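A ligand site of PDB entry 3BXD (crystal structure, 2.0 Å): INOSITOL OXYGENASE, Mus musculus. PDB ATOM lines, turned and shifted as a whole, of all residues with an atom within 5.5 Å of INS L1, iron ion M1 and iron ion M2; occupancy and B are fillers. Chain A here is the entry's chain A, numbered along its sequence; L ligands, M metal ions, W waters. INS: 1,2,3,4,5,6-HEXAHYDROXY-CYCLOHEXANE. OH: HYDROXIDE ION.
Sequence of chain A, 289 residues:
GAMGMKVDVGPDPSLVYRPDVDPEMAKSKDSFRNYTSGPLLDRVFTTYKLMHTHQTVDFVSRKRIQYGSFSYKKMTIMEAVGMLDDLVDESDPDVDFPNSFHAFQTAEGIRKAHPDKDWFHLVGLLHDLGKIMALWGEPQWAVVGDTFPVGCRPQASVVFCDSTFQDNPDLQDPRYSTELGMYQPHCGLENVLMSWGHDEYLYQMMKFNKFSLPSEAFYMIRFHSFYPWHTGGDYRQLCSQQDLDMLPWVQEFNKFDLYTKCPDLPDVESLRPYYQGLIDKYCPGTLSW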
ATOM      1  N   ARG A  33     -15.798 -33.257 -20.418  1.00  0.00           N
ATOM      2  CA  ARG A  33     -14.535 -33.740 -19.893  1.00  0.00           C
ATOM      3  C   ARG A  33     -14.571 -35.257 -19.792  1.00  0.00           C
ATOM      4  O   ARG A  33     -14.155 -35.841 -18.792  1.00  0.00           O
ATOM      5  CB  ARG A  33     -14.292 -33.087 -18.535  1.00  0.00           C
ATOM      6  CG  ARG A  33     -13.120 -33.593 -17.756  1.00  0.00           C
ATOM      7  CD  ARG A  33     -12.512 -32.471 -16.932  1.00  0.00           C
ATOM      8  NE  ARG A  33     -11.589 -31.686 -17.731  1.00  0.00           N
ATOM      9  CZ  ARG A  33     -10.278 -31.893 -17.786  1.00  0.00           C
ATOM     10  NH1 ARG A  33      -9.717 -32.854 -17.055  1.00  0.00           N
ATOM     11  NH2 ARG A  33      -9.519 -31.134 -18.554  1.00  0.00           N
ATOM     12  N   TYR A  35     -13.251 -38.774 -20.779  1.00  0.00           N
ATOM     13  CA  TYR A  35     -12.055 -39.418 -21.296  1.00  0.00           C
ATOM     14  C   TYR A  35     -12.220 -40.925 -21.398  1.00  0.00           C
ATOM     15  O   TYR A  35     -11.252 -41.670 -21.621  1.00  0.00           O
ATOM     16  CB  TYR A  35     -10.850 -39.082 -20.412  1.00  0.00           C
ATOM     17  CG  TYR A  35     -10.544 -37.603 -20.365  1.00  0.00           C
ATOM     18  CD1 TYR A  35     -10.056 -36.951 -21.489  1.00  0.00           C
ATOM     19  CD2 TYR A  35     -10.751 -36.866 -19.208  1.00  0.00           C
ATOM     20  CE1 TYR A  35      -9.774 -35.592 -21.456  1.00  0.00           C
ATOM     21  CE2 TYR A  35     -10.469 -35.513 -19.168  1.00  0.00           C
ATOM     22  CZ  TYR A  35      -9.990 -34.888 -20.290  1.00  0.00           C
ATOM     23  OH  TYR A  35      -9.708 -33.536 -20.250  1.00  0.00           O
ATOM     24  N   TYR A  48      -1.969 -36.601 -25.236  1.00  0.00           N
ATOM     25  CA  TYR A  48      -1.562 -36.577 -23.820  1.00  0.00           C
ATOM     26  C   TYR A  48      -0.493 -37.627 -23.569  1.00  0.00           C
ATOM     27  O   TYR A  48       0.342 -37.497 -22.669  1.00  0.00           O
ATOM     28  CB  TYR A  48      -2.748 -36.863 -22.894  1.00  0.00           C
ATOM     29  CG  TYR A  48      -3.506 -35.632 -22.480  1.00  0.00           C
ATOM     30  CD1 TYR A  48      -2.912 -34.671 -21.665  1.00  0.00           C
ATOM     31  CD2 TYR A  48      -4.810 -35.439 -22.890  1.00  0.00           C
ATOM     32  CE1 TYR A  48      -3.605 -33.539 -21.293  1.00  0.00           C
ATOM     33  CE2 TYR A  48      -5.517 -34.317 -22.515  1.00  0.00           C
ATOM     34  CZ  TYR A  48      -4.899 -33.372 -21.713  1.00  0.00           C
ATOM     35  OH  TYR A  48      -5.600 -32.261 -21.347  1.00  0.00           O
ATOM     36  N   ASP A  89      -7.818 -26.599 -30.576  1.00  0.00           N
ATOM     37  CA  ASP A  89      -7.101 -27.297 -29.507  1.00  0.00           C
ATOM     38  C   ASP A  89      -7.324 -28.816 -29.609  1.00  0.00           C
ATOM     39  O   ASP A  89      -8.464 -29.289 -29.621  1.00  0.00           O
ATOM     40  CB  ASP A  89      -7.552 -26.739 -28.153  1.00  0.00           C
ATOM     41  CG  ASP A  89      -6.727 -27.271 -27.009  1.00  0.00           C
ATOM     42  OD1 ASP A  89      -6.281 -28.431 -27.091  1.00  0.00           O
ATOM     43  OD2 ASP A  89      -6.537 -26.529 -26.018  1.00  0.00           O
ATOM     44  N   SER A  91      -6.289 -31.246 -27.560  1.00  0.00           N
ATOM     45  CA  SER A  91      -6.457 -31.944 -26.292  1.00  0.00           C
ATOM     46  C   SER A  91      -7.872 -31.837 -25.731  1.00  0.00           C
ATOM     47  O   SER A  91      -8.239 -32.585 -24.830  1.00  0.00           O
ATOM     48  CB  SER A  91      -5.486 -31.384 -25.255  1.00  0.00           C
ATOM     49  OG  SER A  91      -5.808 -30.044 -24.951  1.00  0.00           O
ATOM     50  N   ASP A  92      -8.663 -30.902 -26.249  1.00  0.00           N
ATOM     51  CA  ASP A  92      -9.994 -30.624 -25.718  1.00  0.00           C
ATOM     52  C   ASP A  92     -11.042 -31.554 -26.340  1.00  0.00           C
ATOM     53  O   ASP A  92     -11.263 -31.523 -27.546  1.00  0.00           O
ATOM     54  CB  ASP A  92     -10.363 -29.162 -25.993  1.00  0.00           C
ATOM     55  CG  ASP A  92     -11.357 -28.600 -24.984  1.00  0.00           C
ATOM     56  OD1 ASP A  92     -11.954 -29.374 -24.203  1.00  0.00           O
ATOM     57  OD2 ASP A  92     -11.542 -27.360 -24.972  1.00  0.00           O
ATOM     58  N   PRO A  93     -11.698 -32.385 -25.494  1.00  0.00           N
ATOM     59  CA  PRO A  93     -12.724 -33.317 -25.969  1.00  0.00           C
ATOM     60  C   PRO A  93     -14.081 -32.650 -26.192  1.00  0.00           C
ATOM     61  O   PRO A  93     -15.024 -33.320 -26.603  1.00  0.00           O
ATOM     62  CB  PRO A  93     -12.839 -34.342 -24.825  1.00  0.00           C
ATOM     63  CG  PRO A  93     -11.787 -33.951 -23.797  1.00  0.00           C
ATOM     64  CD  PRO A  93     -11.449 -32.524 -24.047  1.00  0.00           C
ATOM     65  N   HIS A 102     -13.804 -19.549 -28.069  1.00  0.00           N
ATOM     66  CA  HIS A 102     -13.824 -20.041 -26.701  1.00  0.00           C
ATOM     67  C   HIS A 102     -13.396 -18.951 -25.718  1.00  0.00           C
ATOM     68  O   HIS A 102     -13.928 -18.873 -24.608  1.00  0.00           O
ATOM     69  CB  HIS A 102     -12.909 -21.257 -26.542  1.00  0.00           C
ATOM     70  CG  HIS A 102     -12.452 -21.489 -25.135  1.00  0.00           C
ATOM     71  ND1 HIS A 102     -13.233 -22.145 -24.197  1.00  0.00           N
ATOM     72  CD2 HIS A 102     -11.304 -21.157 -24.499  1.00  0.00           C
ATOM     73  CE1 HIS A 102     -12.588 -22.193 -23.054  1.00  0.00           C
ATOM     74  NE2 HIS A 102     -11.412 -21.604 -23.205  1.00  0.00           N
ATOM     75  N   THR A 106     -15.880 -17.712 -22.637  1.00  0.00           N
ATOM     76  CA  THR A 106     -15.450 -17.819 -21.254  1.00  0.00           C
ATOM     77  C   THR A 106     -15.583 -16.462 -20.573  1.00  0.00           C
ATOM     78  O   THR A 106     -16.093 -16.354 -19.461  1.00  0.00           O
ATOM     79  CB  THR A 106     -13.992 -18.319 -21.130  1.00  0.00           C
ATOM     80  OG1 THR A 106     -13.885 -19.643 -21.689  1.00  0.00           O
ATOM     81  CG2 THR A 106     -13.556 -18.362 -19.677  1.00  0.00           C
ATOM     82  N   HIS A 127      -7.091 -15.963 -20.923  1.00  0.00           N
ATOM     83  CA  HIS A 127      -6.463 -17.123 -20.256  1.00  0.00           C
ATOM     84  C   HIS A 127      -5.774 -18.117 -21.187  1.00  0.00           C
ATOM     85  O   HIS A 127      -4.793 -18.766 -20.790  1.00  0.00           O
ATOM     86  CB  HIS A 127      -7.488 -17.847 -19.383  1.00  0.00           C
ATOM     87  CG  HIS A 127      -8.430 -18.720 -20.147  1.00  0.00           C
ATOM     88  ND1 HIS A 127      -9.574 -18.229 -20.736  1.00  0.00           N
ATOM     89  CD2 HIS A 127      -8.398 -20.046 -20.420  1.00  0.00           C
ATOM     90  CE1 HIS A 127     -10.205 -19.212 -21.346  1.00  0.00           C
ATOM     91  NE2 HIS A 127      -9.500 -20.328 -21.169  1.00  0.00           N
ATOM     92  N   ASP A 128      -6.260 -18.240 -22.416  1.00  0.00           N
ATOM     93  CA  ASP A 128      -5.705 -19.212 -23.352  1.00  0.00           C
ATOM     94  C   ASP A 128      -4.857 -18.611 -24.480  1.00  0.00           C
ATOM     95  O   ASP A 128      -4.594 -19.292 -25.476  1.00  0.00           O
ATOM     96  CB  ASP A 128      -6.836 -20.028 -23.986  1.00  0.00           C
ATOM     97  CG  ASP A 128      -7.234 -21.210 -23.137  1.00  0.00           C
ATOM     98  OD1 ASP A 128      -6.496 -21.522 -22.180  1.00  0.00           O
ATOM     99  OD2 ASP A 128      -8.273 -21.825 -23.439  1.00  0.00           O
ATOM    100  N   LYS A 131      -1.592 -20.150 -26.244  1.00  0.00           N
ATOM    101  CA  LYS A 131      -1.646 -21.181 -27.292  1.00  0.00           C
ATOM    102  C   LYS A 131      -1.201 -20.655 -28.652  1.00  0.00           C
ATOM    103  O   LYS A 131      -1.195 -21.401 -29.631  1.00  0.00           O
ATOM    104  CB  LYS A 131      -3.066 -21.730 -27.419  1.00  0.00           C
ATOM    105  CG  LYS A 131      -3.549 -22.464 -26.193  1.00  0.00           C
ATOM    106  CD  LYS A 131      -5.023 -22.761 -26.275  1.00  0.00           C
ATOM    107  CE  LYS A 131      -5.507 -23.478 -25.034  1.00  0.00           C
ATOM    108  NZ  LYS A 131      -6.969 -23.711 -25.112  1.00  0.00           N
ATOM    109  N   VAL A 144      -0.851 -27.036 -25.281  1.00  0.00           N
ATOM    110  CA  VAL A 144      -2.172 -27.198 -24.709  1.00  0.00           C
ATOM    111  C   VAL A 144      -2.242 -28.397 -23.770  1.00  0.00           C
ATOM    112  O   VAL A 144      -1.288 -29.166 -23.640  1.00  0.00           O
ATOM    113  CB  VAL A 144      -3.224 -27.409 -25.819  1.00  0.00           C
ATOM    114  CG1 VAL A 144      -3.188 -26.271 -26.816  1.00  0.00           C
ATOM    115  CG2 VAL A 144      -2.999 -28.739 -26.522  1.00  0.00           C
ATOM    116  N   GLY A 145      -3.393 -28.531 -23.108  1.00  0.00           N
ATOM    117  CA  GLY A 145      -3.693 -29.706 -22.311  1.00  0.00           C
ATOM    118  C   GLY A 145      -3.543 -29.503 -20.824  1.00  0.00           C
ATOM    119  O   GLY A 145      -3.021 -28.490 -20.356  1.00  0.00           O
ATOM    120  N   ASP A 146      -4.023 -30.488 -20.060  1.00  0.00           N
ATOM    121  CA  ASP A 146      -3.832 -30.512 -18.623  1.00  0.00           C
ATOM    122  C   ASP A 146      -2.348 -30.527 -18.308  1.00  0.00           C
ATOM    123  O   ASP A 146      -1.551 -31.126 -19.030  1.00  0.00           O
ATOM    124  CB  ASP A 146      -4.463 -31.768 -18.017  1.00  0.00           C
ATOM    125  CG  ASP A 146      -5.975 -31.741 -18.042  1.00  0.00           C
ATOM    126  OD1 ASP A 146      -6.535 -30.701 -18.463  1.00  0.00           O
ATOM    127  OD2 ASP A 146      -6.597 -32.742 -17.638  1.00  0.00           O
ATOM    128  N   THR A 147      -1.990 -29.874 -17.209  1.00  0.00           N
ATOM    129  CA  THR A 147      -0.621 -29.796 -16.781  1.00  0.00           C
ATOM    130  C   THR A 147      -0.396 -30.678 -15.551  1.00  0.00           C
ATOM    131  O   THR A 147      -1.336 -31.088 -14.876  1.00  0.00           O
ATOM    132  CB  THR A 147      -0.259 -28.366 -16.412  1.00  0.00           C
ATOM    133  OG1 THR A 147      -1.266 -27.842 -15.545  1.00  0.00           O
ATOM    134  CG2 THR A 147      -0.166 -27.509 -17.679  1.00  0.00           C
ATOM    135  N   HIS A 198       0.675 -23.252 -22.287  1.00  0.00           N
ATOM    136  CA  HIS A 198       0.121 -21.905 -22.343  1.00  0.00           C
ATOM    137  C   HIS A 198      -0.040 -21.232 -20.986  1.00  0.00           C
ATOM    138  O   HIS A 198       0.015 -20.004 -20.898  1.00  0.00           O
ATOM    139  CB  HIS A 198      -1.216 -21.932 -23.084  1.00  0.00           C
ATOM    140  CG  HIS A 198      -2.274 -22.751 -22.406  1.00  0.00           C
ATOM    141  ND1 HIS A 198      -2.162 -24.108 -22.233  1.00  0.00           N
ATOM    142  CD2 HIS A 198      -3.478 -22.404 -21.898  1.00  0.00           C
ATOM    143  CE1 HIS A 198      -3.243 -24.561 -21.634  1.00  0.00           C
ATOM    144  NE2 HIS A 198      -4.064 -23.543 -21.412  1.00  0.00           N
ATOM    145  N   ASP A 199      -0.214 -22.029 -19.925  1.00  0.00           N
ATOM    146  CA  ASP A 199      -0.412 -21.487 -18.580  1.00  0.00           C
ATOM    147  C   ASP A 199       0.784 -20.676 -18.172  1.00  0.00           C
ATOM    148  O   ASP A 199       0.681 -19.478 -17.924  1.00  0.00           O
ATOM    149  CB  ASP A 199      -0.566 -22.590 -17.535  1.00  0.00           C
ATOM    150  CG  ASP A 199      -1.918 -23.241 -17.545  1.00  0.00           C
ATOM    151  OD1 ASP A 199      -2.536 -23.278 -18.628  1.00  0.00           O
ATOM    152  OD2 ASP A 199      -2.356 -23.712 -16.471  1.00  0.00           O
ATOM    153  N   HIS A 224      -4.599 -22.764 -14.270  1.00  0.00           N
ATOM    154  CA  HIS A 224      -5.962 -23.125 -14.666  1.00  0.00           C
ATOM    155  C   HIS A 224      -6.029 -24.486 -15.366  1.00  0.00           C
ATOM    156  O   HIS A 224      -7.088 -25.115 -15.402  1.00  0.00           O
ATOM    157  CB  HIS A 224      -6.581 -22.040 -15.560  1.00  0.00           C
ATOM    158  CG  HIS A 224      -6.141 -22.109 -16.990  1.00  0.00           C
ATOM    159  ND1 HIS A 224      -5.049 -21.418 -17.472  1.00  0.00           N
ATOM    160  CD2 HIS A 224      -6.641 -22.794 -18.048  1.00  0.00           C
ATOM    161  CE1 HIS A 224      -4.907 -21.660 -18.758  1.00  0.00           C
ATOM    162  NE2 HIS A 224      -5.859 -22.510 -19.127  1.00  0.00           N
ATOM    163  N   SER A 225      -4.907 -24.935 -15.890  1.00  0.00           N
ATOM    164  CA  SER A 225      -4.829 -26.230 -16.574  1.00  0.00           C
ATOM    165  C   SER A 225      -4.488 -27.375 -15.622  1.00  0.00           C
ATOM    166  O   SER A 225      -4.493 -28.536 -16.019  1.00  0.00           O
ATOM    167  CB  SER A 225      -3.771 -26.171 -17.670  1.00  0.00           C
ATOM    168  OG  SER A 225      -4.012 -25.107 -18.580  1.00  0.00           O
ATOM    169  N   PHE A 226      -4.197 -27.046 -14.372  1.00  0.00           N
ATOM    170  CA  PHE A 226      -3.643 -28.008 -13.429  1.00  0.00           C
ATOM    171  C   PHE A 226      -4.759 -28.831 -12.758  1.00  0.00           C
ATOM    172  O   PHE A 226      -4.959 -28.770 -11.544  1.00  0.00           O
ATOM    173  CB  PHE A 226      -2.782 -27.263 -12.397  1.00  0.00           C
ATOM    174  CG  PHE A 226      -1.924 -28.161 -11.547  1.00  0.00           C
ATOM    175  CD1 PHE A 226      -1.815 -29.511 -11.823  1.00  0.00           C
ATOM    176  CD2 PHE A 226      -1.210 -27.642 -10.486  1.00  0.00           C
ATOM    177  CE1 PHE A 226      -1.024 -30.334 -11.045  1.00  0.00           C
ATOM    178  CE2 PHE A 226      -0.415 -28.464  -9.694  1.00  0.00           C
ATOM    179  CZ  PHE A 226      -0.315 -29.799  -9.983  1.00  0.00           C
ATOM    180  N   TYR A 227      -5.465 -29.614 -13.571  1.00  0.00           N
ATOM    181  CA  TYR A 227      -6.656 -30.308 -13.140  1.00  0.00           C
ATOM    182  C   TYR A 227      -6.390 -31.270 -11.991  1.00  0.00           C
ATOM    183  O   TYR A 227      -7.136 -31.277 -11.026  1.00  0.00           O
ATOM    184  CB  TYR A 227      -7.310 -31.057 -14.306  1.00  0.00           C
ATOM    185  CG  TYR A 227      -8.334 -30.231 -15.059  1.00  0.00           C
ATOM    186  CD1 TYR A 227      -7.939 -29.279 -16.005  1.00  0.00           C
ATOM    187  CD2 TYR A 227      -9.691 -30.396 -14.828  1.00  0.00           C
ATOM    188  CE1 TYR A 227      -8.877 -28.529 -16.697  1.00  0.00           C
ATOM    189  CE2 TYR A 227     -10.638 -29.642 -15.518  1.00  0.00           C
ATOM    190  CZ  TYR A 227     -10.227 -28.716 -16.446  1.00  0.00           C
ATOM    191  OH  TYR A 227     -11.155 -27.969 -17.140  1.00  0.00           O
ATOM    192  N   ASP A 257     -14.571 -21.830 -17.500  1.00  0.00           N
ATOM    193  CA  ASP A 257     -13.602 -22.200 -18.527  1.00  0.00           C
ATOM    194  C   ASP A 257     -14.154 -23.406 -19.261  1.00  0.00           C
ATOM    195  O   ASP A 257     -14.161 -23.467 -20.478  1.00  0.00           O
ATOM    196  CB  ASP A 257     -12.242 -22.517 -17.873  1.00  0.00           C
ATOM    197  CG  ASP A 257     -11.188 -22.971 -18.875  1.00  0.00           C
ATOM    198  OD1 ASP A 257     -11.341 -22.708 -20.085  1.00  0.00           O
ATOM    199  OD2 ASP A 257     -10.189 -23.593 -18.439  1.00  0.00           O
ATOM    200  N   LYS A 261     -18.216 -23.910 -22.919  1.00  0.00           N
ATOM    201  CA  LYS A 261     -17.886 -24.470 -24.230  1.00  0.00           C
ATOM    202  C   LYS A 261     -19.144 -24.968 -24.954  1.00  0.00           C
ATOM    203  O   LYS A 261     -19.809 -25.889 -24.482  1.00  0.00           O
ATOM    204  CB  LYS A 261     -16.845 -25.594 -24.087  1.00  0.00           C
ATOM    205  CG  LYS A 261     -15.439 -25.090 -23.761  1.00  0.00           C
ATOM    206  CD  LYS A 261     -14.524 -26.210 -23.276  1.00  0.00           C
ATOM    207  CE  LYS A 261     -13.168 -25.672 -22.844  1.00  0.00           C
ATOM    208  NZ  LYS A 261     -12.306 -26.701 -22.203  1.00  0.00           N
HETATM  209  C1  INS L   1      -7.480 -25.801 -21.865  1.00  0.00           C
HETATM  210  C2  INS L   1      -7.557 -26.948 -22.885  1.00  0.00           C
HETATM  211  C3  INS L   1      -8.099 -28.205 -22.219  1.00  0.00           C
HETATM  212  C4  INS L   1      -7.174 -28.599 -21.079  1.00  0.00           C
HETATM  213  C5  INS L   1      -7.093 -27.474 -20.053  1.00  0.00           C
HETATM  214  C6  INS L   1      -6.553 -26.207 -20.696  1.00  0.00           C
HETATM  215  O1  INS L   1      -6.966 -24.644 -22.501  1.00  0.00           O
HETATM  216  O2  INS L   1      -6.257 -27.211 -23.431  1.00  0.00           O
HETATM  217  O3  INS L   1      -8.131 -29.265 -23.171  1.00  0.00           O
HETATM  218  O4  INS L   1      -7.729 -29.743 -20.449  1.00  0.00           O
HETATM  219  O5  INS L   1      -6.242 -27.887 -18.975  1.00  0.00           O
HETATM  220  O6  INS L   1      -6.468 -25.157 -19.735  1.00  0.00           O
HETATM  221  O    OH L   2      -8.653 -23.546 -20.271  1.00  0.00           O
HETATM  222 FE    FE M   1      -9.703 -22.361 -21.778  1.00  0.00          FE
HETATM  223 FE    FE M   2      -6.414 -23.347 -21.006  1.00  0.00          FE
HETATM  224  O   HOH W   1     -10.057 -24.268 -22.955  1.00  0.00           O
HETATM  225  O   HOH W   2      -7.920 -31.952 -22.495  1.00  0.00           O
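The guanidinium group (NH2) of Arg 33 sits at hydrogen-bond distance from an oxygen (O4) of INS L1. O6 of INS L1 sits close to OG of Ser 225. The backbone NH of Gly 145 sits at hydrogen-bond distance from an oxygen (O2) of INS L1 (3.2 Å). O4 of INS L1 is in hydrogen-bond range of OD1 of Asp 146 (2.5 Å). OH of Tyr 48 lies within hydrogen-bond range of O4 of INS L1, 3.4 Å away. O of Ser 225 sits close to O5 of INS L1, 3.5 Å away. The side-chain carboxylate (OD2) of Asp 89 is in hydrogen-bond range of an oxygen (O2) of INS L1 (2.7 Å). The side-chain amino group (NZ) of Lys 131 sits close to an oxygen (O1) of INS L1 (2.8 Å). O3 of INS L1 sits at hydrogen-bond distance from OG of Ser 91, 3.0 Å away.
The side-chain hydroxyl (OG) of Ser 91 lies within hydrogen-bond range of the backbone NH (N) of Gly 145 (3.4 Å). The backbone carbonyl oxygen (O) of Ser 225 sits at hydrogen-bond distance from the backbone NH (N) of Thr 147 (3.1 Å). OD1 of Asp 199 lies close to NE2 of His 198 (3.2 Å). A ring nitrogen (NE2) of His 224 sits close to the side-chain hydroxyl (OG) of Ser 225, at 3.2 Å. The backbone NH (N) of Ser 225 lies within hydrogen-bond range of the side-chain carboxylate (OD2) of Asp 199, at 2.9 Å. OD2 of Asp 128 sits close to NZ of Lys 131, 2.8 Å away. The backbone NH of His 224 is in hydrogen-bond range of the side-chain carboxylate of Asp 199 (3.3 Å). NZ of Lys 261 is in salt-bridge range of OD2 of Asp 92, at 2.9 Å.
CA of Asp 92 touches O3 of INS L1, 3.4 Å away. Val 144 touches INS L1 (CB to O2, 3.9 Å). CE1 of Tyr 227 touches O5 of INS L1, 3.5 Å away. Hydrophobic or aromatic side chains that line INS L1: Val 144, His 198, His 224 and Tyr 227. Of the 24 residues printed, 14 come within 4 Å of INS L1. Along chain A the residues within 4 Å of INS L1 span positions 33 to 227.
Of the 24 residues printed, 4 come within 4 Å of iron ion M1. The nearest printed residue that does not touch iron ion M1 is Lys 131 (4.5 Å).
Ser 225 touches iron ion M2. Five residues have an atom within 4 Å of iron ion M2: His 127, Asp 128, His 198, His 224 and Ser 225.
A ring nitrogen (NE2) of His 127 is bound to iron ion M1, at 2.1 Å. O of OH L2 is bound to iron ion M1. OD2 of Asp 128 binds iron ion M1, at 2.3 Å. Water W1 is bound to iron ion M1, 2.3 Å away. NE2 of His 102 is bound to iron ion M1 (2.4 Å). OD1 of Asp 257 binds iron ion M1 (2.4 Å). Iron ion M1 has six donor atoms within binding distance.
Iron ion M2 is bound by an oxygen (O1) of INS L1 (2.1 Å), a ring nitrogen (NE2) of His 224 (2.1 Å), the side-chain carboxylate of Asp 128 (2.2 Å), an oxygen (O6) of INS L1 (2.2 Å), an oxygen (O) of OH L2 (2.4 Å) and a ring nitrogen (NE2) of His 198 (2.4 Å). Iron ion M2 has six donor atoms within binding distance.
Water W2 lies within hydrogen-bond range of the backbone carbonyl oxygen of Ser 91 (2.4 Å), the side-chain hydroxyl of Tyr 48 (2.6 Å), an oxygen (O3) of INS L1 (2.8 Å) and the side-chain hydroxyl of Tyr 35 (3.3 Å).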
